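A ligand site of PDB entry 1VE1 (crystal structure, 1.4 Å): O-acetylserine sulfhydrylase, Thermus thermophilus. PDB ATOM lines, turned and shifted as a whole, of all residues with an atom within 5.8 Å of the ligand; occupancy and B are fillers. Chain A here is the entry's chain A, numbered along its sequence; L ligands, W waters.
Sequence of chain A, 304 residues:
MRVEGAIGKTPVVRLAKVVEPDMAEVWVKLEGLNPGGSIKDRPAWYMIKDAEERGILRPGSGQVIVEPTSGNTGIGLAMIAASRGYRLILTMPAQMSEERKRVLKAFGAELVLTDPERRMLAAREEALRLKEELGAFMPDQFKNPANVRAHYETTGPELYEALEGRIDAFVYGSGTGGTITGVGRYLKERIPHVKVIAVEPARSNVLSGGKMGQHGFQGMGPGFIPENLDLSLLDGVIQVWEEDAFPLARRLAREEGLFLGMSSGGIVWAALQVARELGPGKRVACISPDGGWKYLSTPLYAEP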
ATOM      1  N   SER A  38      11.484 -16.914  17.555  1.00  0.00           N
ATOM      2  CA  SER A  38      12.620 -17.607  18.163  1.00  0.00           C
ATOM      3  C   SER A  38      13.574 -18.224  17.169  1.00  0.00           C
ATOM      4  O   SER A  38      13.319 -18.269  15.959  1.00  0.00           O
ATOM      5  CB  SER A  38      12.119 -18.721  19.089  1.00  0.00           C
ATOM      6  OG  SER A  38      11.870 -19.905  18.333  1.00  0.00           O
ATOM      7  N   ILE A  39      14.677 -18.710  17.707  1.00  0.00           N
ATOM      8  CA  ILE A  39      15.721 -19.368  16.934  1.00  0.00           C
ATOM      9  C   ILE A  39      15.179 -20.625  16.240  1.00  0.00           C
ATOM     10  O   ILE A  39      15.720 -21.052  15.226  1.00  0.00           O
ATOM     11  CB  ILE A  39      16.895 -19.746  17.875  1.00  0.00           C
ATOM     12  CG1 ILE A  39      18.084 -20.254  17.066  1.00  0.00           C
ATOM     13  CG2 ILE A  39      16.438 -20.791  18.891  1.00  0.00           C
ATOM     14  CD1 ILE A  39      19.340 -20.452  17.897  1.00  0.00           C
ATOM     15  N   LYS A  40      14.109 -21.197  16.787  1.00  0.00           N
ATOM     16  CA  LYS A  40      13.541 -22.415  16.200  1.00  0.00           C
ATOM     17  C   LYS A  40      12.992 -22.246  14.803  1.00  0.00           C
ATOM     18  O   LYS A  40      12.703 -23.239  14.128  1.00  0.00           O
ATOM     19  CB  LYS A  40      12.453 -22.991  17.108  1.00  0.00           C
ATOM     20  CG  LYS A  40      12.968 -23.550  18.411  1.00  0.00           C
ATOM     21  CD  LYS A  40      13.952 -24.692  18.201  1.00  0.00           C
ATOM     22  CE  LYS A  40      13.959 -25.598  19.427  1.00  0.00           C
ATOM     23  NZ  LYS A  40      13.952 -24.689  20.586  1.00  0.00           N
ATOM     24  N   ASN A  72       8.796 -23.496  21.129  1.00  0.00           N
ATOM     25  CA  ASN A  72       9.207 -22.712  19.977  1.00  0.00           C
ATOM     26  C   ASN A  72       9.254 -23.511  18.681  1.00  0.00           C
ATOM     27  O   ASN A  72       8.954 -22.978  17.624  1.00  0.00           O
ATOM     28  CB  ASN A  72      10.555 -22.038  20.238  1.00  0.00           C
ATOM     29  CG  ASN A  72      10.429 -20.815  21.124  1.00  0.00           C
ATOM     30  OD1 ASN A  72       9.455 -20.058  21.018  1.00  0.00           O
ATOM     31  ND2 ASN A  72      11.411 -20.602  21.982  1.00  0.00           N
ATOM     32  N   THR A  73       9.631 -24.783  18.750  1.00  0.00           N
ATOM     33  CA  THR A  73       9.659 -25.582  17.529  1.00  0.00           C
ATOM     34  C   THR A  73       8.232 -25.727  17.007  1.00  0.00           C
ATOM     35  O   THR A  73       8.003 -25.707  15.804  1.00  0.00           O
ATOM     36  CB  THR A  73      10.268 -26.969  17.786  1.00  0.00           C
ATOM     37  OG1 THR A  73      11.642 -26.812  18.159  1.00  0.00           O
ATOM     38  CG2 THR A  73      10.205 -27.822  16.526  1.00  0.00           C
ATOM     39  N   GLN A 141      12.792 -33.311  15.800  1.00  0.00           N
ATOM     40  CA  GLN A 141      13.773 -32.278  16.122  1.00  0.00           C
ATOM     41  C   GLN A 141      15.025 -32.666  16.893  1.00  0.00           C
ATOM     42  O   GLN A 141      16.064 -32.035  16.726  1.00  0.00           O
ATOM     43  CB  GLN A 141      13.078 -31.115  16.840  1.00  0.00           C
ATOM     44  CG  GLN A 141      12.662 -31.428  18.269  1.00  0.00           C
ATOM     45  CD  GLN A 141      12.144 -30.199  18.978  1.00  0.00           C
ATOM     46  OE1 GLN A 141      12.686 -29.110  18.803  1.00  0.00           O
ATOM     47  NE2 GLN A 141      11.113 -30.368  19.791  1.00  0.00           N
ATOM     48  N   ASN A 147      18.363 -30.067  11.376  1.00  0.00           N
ATOM     49  CA  ASN A 147      18.282 -29.109  12.471  1.00  0.00           C
ATOM     50  C   ASN A 147      19.681 -28.520  12.634  1.00  0.00           C
ATOM     51  O   ASN A 147      19.879 -27.307  12.568  1.00  0.00           O
ATOM     52  CB  ASN A 147      17.843 -29.852  13.751  1.00  0.00           C
ATOM     53  CG  ASN A 147      17.808 -28.960  14.985  1.00  0.00           C
ATOM     54  OD1 ASN A 147      18.476 -27.941  15.038  1.00  0.00           O
ATOM     55  ND2 ASN A 147      17.062 -29.395  15.999  1.00  0.00           N
ATOM     56  N   HIS A 151      21.898 -24.392  11.429  1.00  0.00           N
ATOM     57  CA  HIS A 151      22.834 -23.551  12.148  1.00  0.00           C
ATOM     58  C   HIS A 151      24.239 -23.546  11.556  1.00  0.00           C
ATOM     59  O   HIS A 151      24.952 -22.549  11.658  1.00  0.00           O
ATOM     60  CB  HIS A 151      22.834 -23.964  13.616  1.00  0.00           C
ATOM     61  CG  HIS A 151      21.516 -23.731  14.279  1.00  0.00           C
ATOM     62  ND1 HIS A 151      20.662 -24.756  14.640  1.00  0.00           N
ATOM     63  CD2 HIS A 151      20.854 -22.585  14.554  1.00  0.00           C
ATOM     64  CE1 HIS A 151      19.537 -24.244  15.117  1.00  0.00           C
ATOM     65  NE2 HIS A 151      19.626 -22.919  15.066  1.00  0.00           N
ATOM     66  N   TYR A 172      26.206 -21.419  24.727  1.00  0.00           N
ATOM     67  CA  TYR A 172      24.799 -21.625  24.399  1.00  0.00           C
ATOM     68  C   TYR A 172      24.094 -22.635  25.283  1.00  0.00           C
ATOM     69  O   TYR A 172      24.673 -23.643  25.672  1.00  0.00           O
ATOM     70  CB  TYR A 172      24.664 -22.064  22.935  1.00  0.00           C
ATOM     71  CG  TYR A 172      23.242 -22.043  22.457  1.00  0.00           C
ATOM     72  CD1 TYR A 172      22.577 -20.828  22.250  1.00  0.00           C
ATOM     73  CD2 TYR A 172      22.538 -23.227  22.229  1.00  0.00           C
ATOM     74  CE1 TYR A 172      21.246 -20.795  21.837  1.00  0.00           C
ATOM     75  CE2 TYR A 172      21.203 -23.203  21.816  1.00  0.00           C
ATOM     76  CZ  TYR A 172      20.569 -21.981  21.626  1.00  0.00           C
ATOM     77  OH  TYR A 172      19.262 -21.949  21.217  1.00  0.00           O
ATOM     78  N   GLY A 173      22.825 -22.357  25.590  1.00  0.00           N
ATOM     79  CA  GLY A 173      22.011 -23.245  26.411  1.00  0.00           C
ATOM     80  C   GLY A 173      21.315 -24.248  25.518  1.00  0.00           C
ATOM     81  O   GLY A 173      20.323 -23.945  24.868  1.00  0.00           O
ATOM     82  N   SER A 174      21.837 -25.473  25.503  1.00  0.00           N
ATOM     83  CA  SER A 174      21.342 -26.534  24.634  1.00  0.00           C
ATOM     84  C   SER A 174      19.965 -27.123  24.918  1.00  0.00           C
ATOM     85  O   SER A 174      19.617 -27.411  26.059  1.00  0.00           O
ATOM     86  CB  SER A 174      22.384 -27.645  24.575  1.00  0.00           C
ATOM     87  OG  SER A 174      22.161 -28.503  23.474  1.00  0.00           O
ATOM     88  N   GLY A 175      19.201 -27.308  23.842  1.00  0.00           N
ATOM     89  CA  GLY A 175      17.884 -27.911  23.910  1.00  0.00           C
ATOM     90  C   GLY A 175      17.977 -29.161  23.049  1.00  0.00           C
ATOM     91  O   GLY A 175      18.242 -30.253  23.552  1.00  0.00           O
ATOM     92  N   THR A 176      17.790 -29.008  21.739  1.00  0.00           N
ATOM     93  CA  THR A 176      17.892 -30.141  20.818  1.00  0.00           C
ATOM     94  C   THR A 176      19.352 -30.427  20.475  1.00  0.00           C
ATOM     95  O   THR A 176      19.672 -31.505  19.982  1.00  0.00           O
ATOM     96  CB  THR A 176      17.149 -29.882  19.476  1.00  0.00           C
ATOM     97  OG1 THR A 176      17.802 -28.818  18.775  1.00  0.00           O
ATOM     98  CG2 THR A 176      15.695 -29.521  19.723  1.00  0.00           C
ATOM     99  N   GLY A 177      20.224 -29.453  20.724  1.00  0.00           N
ATOM    100  CA  GLY A 177      21.631 -29.622  20.416  1.00  0.00           C
ATOM    101  C   GLY A 177      22.003 -29.083  19.042  1.00  0.00           C
ATOM    102  O   GLY A 177      23.182 -28.966  18.712  1.00  0.00           O
ATOM    103  N   GLY A 178      21.002 -28.745  18.237  1.00  0.00           N
ATOM    104  CA  GLY A 178      21.268 -28.252  16.898  1.00  0.00           C
ATOM    105  C   GLY A 178      22.117 -27.003  16.800  1.00  0.00           C
ATOM    106  O   GLY A 178      23.054 -26.943  16.003  1.00  0.00           O
ATOM    107  N   THR A 179      21.793 -25.995  17.612  1.00  0.00           N
ATOM    108  CA  THR A 179      22.532 -24.746  17.580  1.00  0.00           C
ATOM    109  C   THR A 179      23.987 -24.865  17.991  1.00  0.00           C
ATOM    110  O   THR A 179      24.881 -24.420  17.278  1.00  0.00           O
ATOM    111  CB  THR A 179      21.848 -23.685  18.478  1.00  0.00           C
ATOM    112  OG1 THR A 179      20.526 -23.444  18.010  1.00  0.00           O
ATOM    113  CG2 THR A 179      22.636 -22.371  18.442  1.00  0.00           C
ATOM    114  N   ILE A 180      24.241 -25.462  19.153  1.00  0.00           N
ATOM    115  CA  ILE A 180      25.622 -25.565  19.597  1.00  0.00           C
ATOM    116  C   ILE A 180      26.461 -26.447  18.686  1.00  0.00           C
ATOM    117  O   ILE A 180      27.642 -26.182  18.478  1.00  0.00           O
ATOM    118  CB  ILE A 180      25.690 -26.024  21.088  1.00  0.00           C
ATOM    119  CG1 ILE A 180      27.040 -25.635  21.685  1.00  0.00           C
ATOM    120  CG2 ILE A 180      25.442 -27.514  21.182  1.00  0.00           C
ATOM    121  CD1 ILE A 180      27.069 -25.635  23.199  1.00  0.00           C
ATOM    122  N   GLN A 218      12.509 -22.530  30.021  1.00  0.00           N
ATOM    123  CA  GLN A 218      11.759 -23.039  28.883  1.00  0.00           C
ATOM    124  C   GLN A 218      12.551 -23.040  27.582  1.00  0.00           C
ATOM    125  O   GLN A 218      13.166 -22.038  27.212  1.00  0.00           O
ATOM    126  CB  GLN A 218      10.464 -22.242  28.706  1.00  0.00           C
ATOM    127  CG  GLN A 218       9.620 -22.159  29.970  1.00  0.00           C
ATOM    128  CD  GLN A 218       8.240 -21.579  29.730  1.00  0.00           C
ATOM    129  OE1 GLN A 218       7.563 -21.140  30.665  1.00  0.00           O
ATOM    130  NE2 GLN A 218       7.804 -21.566  28.471  1.00  0.00           N
ATOM    131  N   GLY A 219      12.553 -24.183  26.898  1.00  0.00           N
ATOM    132  CA  GLY A 219      13.259 -24.285  25.640  1.00  0.00           C
ATOM    133  C   GLY A 219      14.619 -24.961  25.692  1.00  0.00           C
ATOM    134  O   GLY A 219      15.101 -25.437  24.670  1.00  0.00           O
ATOM    135  N   MET A 220      15.240 -24.993  26.863  1.00  0.00           N
ATOM    136  CA  MET A 220      16.559 -25.634  26.988  1.00  0.00           C
ATOM    137  C   MET A 220      16.545 -26.656  28.117  1.00  0.00           C
ATOM    138  O   MET A 220      15.605 -26.704  28.909  1.00  0.00           O
ATOM    139  CB  MET A 220      17.645 -24.590  27.237  1.00  0.00           C
ATOM    140  CG  MET A 220      17.551 -23.844  28.558  1.00  0.00           C
ATOM    141  SD  MET A 220      18.950 -22.724  28.843  1.00  0.00           S
ATOM    142  CE  MET A 220      20.132 -23.855  29.535  1.00  0.00           C
ATOM    143  N   SER A 263      15.481 -18.722  28.914  1.00  0.00           N
ATOM    144  CA  SER A 263      16.748 -19.370  28.587  1.00  0.00           C
ATOM    145  C   SER A 263      17.862 -18.352  28.344  1.00  0.00           C
ATOM    146  O   SER A 263      19.033 -18.645  28.574  1.00  0.00           O
ATOM    147  CB  SER A 263      16.584 -20.294  27.375  1.00  0.00           C
ATOM    148  OG  SER A 263      16.239 -19.561  26.205  1.00  0.00           O
ATOM    149  N   ILE A 267      21.703 -18.337  29.704  1.00  0.00           N
ATOM    150  CA  ILE A 267      22.798 -18.317  28.737  1.00  0.00           C
ATOM    151  C   ILE A 267      23.718 -17.120  28.962  1.00  0.00           C
ATOM    152  O   ILE A 267      24.931 -17.271  28.971  1.00  0.00           O
ATOM    153  CB  ILE A 267      22.238 -18.312  27.304  1.00  0.00           C
ATOM    154  CG1 ILE A 267      21.562 -19.658  27.027  1.00  0.00           C
ATOM    155  CG2 ILE A 267      23.356 -18.046  26.290  1.00  0.00           C
ATOM    156  CD1 ILE A 267      20.812 -19.721  25.719  1.00  0.00           C
ATOM    157  N   PRO A 289      17.874 -17.209  22.523  1.00  0.00           N
ATOM    158  CA  PRO A 289      16.885 -17.980  21.758  1.00  0.00           C
ATOM    159  C   PRO A 289      15.586 -17.263  21.434  1.00  0.00           C
ATOM    160  O   PRO A 289      15.031 -17.443  20.342  1.00  0.00           O
ATOM    161  CB  PRO A 289      16.671 -19.208  22.635  1.00  0.00           C
ATOM    162  CG  PRO A 289      18.004 -19.372  23.305  1.00  0.00           C
ATOM    163  CD  PRO A 289      18.336 -17.969  23.702  1.00  0.00           C
ATOM    164  N   ASP A 290      15.086 -16.465  22.369  1.00  0.00           N
ATOM    165  CA  ASP A 290      13.857 -15.715  22.115  1.00  0.00           C
ATOM    166  C   ASP A 290      13.709 -14.536  23.052  1.00  0.00           C
ATOM    167  O   ASP A 290      14.509 -14.373  23.985  1.00  0.00           O
ATOM    168  CB  ASP A 290      12.614 -16.627  22.140  1.00  0.00           C
ATOM    169  CG  ASP A 290      12.342 -17.275  23.493  1.00  0.00           C
ATOM    170  OD1 ASP A 290      11.354 -18.048  23.544  1.00  0.00           O
ATOM    171  OD2 ASP A 290      13.051 -17.042  24.479  1.00  0.00           O
ATOM    172  N   TYR A 295       6.629 -14.700  27.867  1.00  0.00           N
ATOM    173  CA  TYR A 295       6.782 -15.002  29.282  1.00  0.00           C
ATOM    174  C   TYR A 295       6.321 -13.974  30.309  1.00  0.00           C
ATOM    175  O   TYR A 295       6.817 -13.954  31.445  1.00  0.00           O
ATOM    176  CB  TYR A 295       8.253 -15.359  29.527  1.00  0.00           C
ATOM    177  CG  TYR A 295       8.800 -16.329  28.498  1.00  0.00           C
ATOM    178  CD1 TYR A 295       9.677 -15.906  27.485  1.00  0.00           C
ATOM    179  CD2 TYR A 295       8.437 -17.672  28.517  1.00  0.00           C
ATOM    180  CE1 TYR A 295      10.164 -16.799  26.526  1.00  0.00           C
ATOM    181  CE2 TYR A 295       8.914 -18.571  27.567  1.00  0.00           C
ATOM    182  CZ  TYR A 295       9.781 -18.130  26.578  1.00  0.00           C
ATOM    183  OH  TYR A 295      10.266 -19.022  25.655  1.00  0.00           O
HETATM  184  N1  LIG L   1      15.998 -21.789  24.376  1.00  0.00           N
HETATM  185  C1  LIG L   1      14.768 -21.745  23.777  1.00  0.00           C
HETATM  186  C2  LIG L   1      13.742 -20.731  24.301  1.00  0.00           C
HETATM  187  C3  LIG L   1      14.486 -22.593  22.722  1.00  0.00           C
HETATM  188  O1  LIG L   1      13.260 -22.573  22.121  1.00  0.00           O
HETATM  189  C4  LIG L   1      15.453 -23.484  22.278  1.00  0.00           C
HETATM  190  C5  LIG L   1      15.155 -24.439  21.126  1.00  0.00           C
HETATM  191  C6  LIG L   1      16.708 -23.518  22.902  1.00  0.00           C
HETATM  192  C7  LIG L   1      16.964 -22.668  23.940  1.00  0.00           C
HETATM  193  C8  LIG L   1      17.859 -24.481  22.477  1.00  0.00           C
HETATM  194  O2  LIG L   1      18.288 -24.444  21.067  1.00  0.00           O
HETATM  195  P1  LIG L   1      18.660 -25.834  20.372  1.00  0.00           P
HETATM  196  O3  LIG L   1      17.429 -26.633  20.229  1.00  0.00           O
HETATM  197  O4  LIG L   1      19.287 -25.561  18.981  1.00  0.00           O
HETATM  198  O5  LIG L   1      19.692 -26.444  21.243  1.00  0.00           O
HETATM  199  O   HOH W   1      10.760 -23.598  23.290  1.00  0.00           O
HETATM  200  O   HOH W   2      17.832 -25.791  16.704  1.00  0.00           O
HETATM  201  O   HOH W   3      22.337 -26.502  21.176  1.00  0.00           O
HETATM  202  O   HOH W   4      13.073 -19.255  27.324  1.00  0.00           O
HETATM  203  O   HOH W   5      14.661 -27.316  22.789  1.00  0.00           O
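NZ of Lys 40 is covalently linked to C5 of the ligand, at 1.3 Å.
The backbone NH of Thr 179 sits at hydrogen-bond distance from an oxygen (O4) of the ligand (2.9 Å).
The side-chain hydroxyl of Thr 179 is in hydrogen-bond range of an oxygen (O4) of the ligand (2.6 Å).
The backbone NH (N) of Thr 176 lies within hydrogen-bond range of an oxygen (O3) of the ligand (2.8 Å).
OG1 of Thr 176 sits at hydrogen-bond distance from O3 of the ligand, 2.7 Å away.
OH of Tyr 172 sits at hydrogen-bond distance from O2 of the ligand (2.7 Å).
O1 of the ligand sits at hydrogen-bond distance from ND2 of Asn 72 (2.7 Å).
O5 of the ligand lies within hydrogen-bond range of N of Gly 175 (2.8 Å).
The side-chain hydroxyl (OG) of Ser 263 lies within hydrogen-bond range of a nitrogen (N1) of the ligand (2.9 Å).
O5 of the ligand is in hydrogen-bond range of N of Gly 177.
The side-chain hydroxyl of Ser 38 is in hydrogen-bond range of the backbone NH of Lys 40 (3.0 Å).
NE2 of His 151 is in hydrogen-bond range of OG1 of Thr 179.
OG1 of Thr 176 sits at hydrogen-bond distance from N of Gly 178 (3.2 Å).
The side-chain amide nitrogen (ND2) of Asn 147 sits at hydrogen-bond distance from the side-chain hydroxyl (OG1) of Thr 176.
ND2 of Asn 72 sits at hydrogen-bond distance from OD1 of Asp 290 (3.0 Å).
OG of Ser 174 lies close to N of Gly 177.
The backbone NH (N) of Ile 39 lies within hydrogen-bond range of the backbone carbonyl oxygen (O) of Pro 289, at 2.9 Å.
The side-chain hydroxyl (OH) of Tyr 295 lies within hydrogen-bond range of the side-chain carboxylate (OD1) of Asp 290 (2.6 Å).
Gly 173 touches the ligand (O to C8, 3.5 Å).
C of Ser 174 touches O5 of the ligand, at 3.7 Å.
N of Gly 178 touches O4 of the ligand, 3.7 Å away.
Gln 218 touches the ligand.
O of Gly 219 touches C6 of the ligand, 3.1 Å away.
CB of Met 220 touches C7 of the ligand, 3.9 Å away.
Pro 289 touches the ligand.
OD1 of Asp 290 touches C2 of the ligand, at 3.7 Å.
Hydrophobic or aromatic side chains within 4 Å of the ligand: Tyr 172, Met 220 and Pro 289.
The nearest printed residue that does not touch the ligand is His 151 (4.1 Å).
Water W3 lies within hydrogen-bond range of O5 of the ligand, N of Ile 180 and OG of Ser 174.
Water W2 bridges an oxygen (O4) of the ligand (2.7 Å) and the side-chain amide oxygen of Asn 147 (2.8 Å).
Water W1 lies within hydrogen-bond range of the backbone NH (N) of Asn 72 (2.9 Å) and an oxygen (O1) of the ligand (2.9 Å).
Water W4 lies within hydrogen-bond range of O of Gln 218, N of Ser 263 and OH of Tyr 295.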
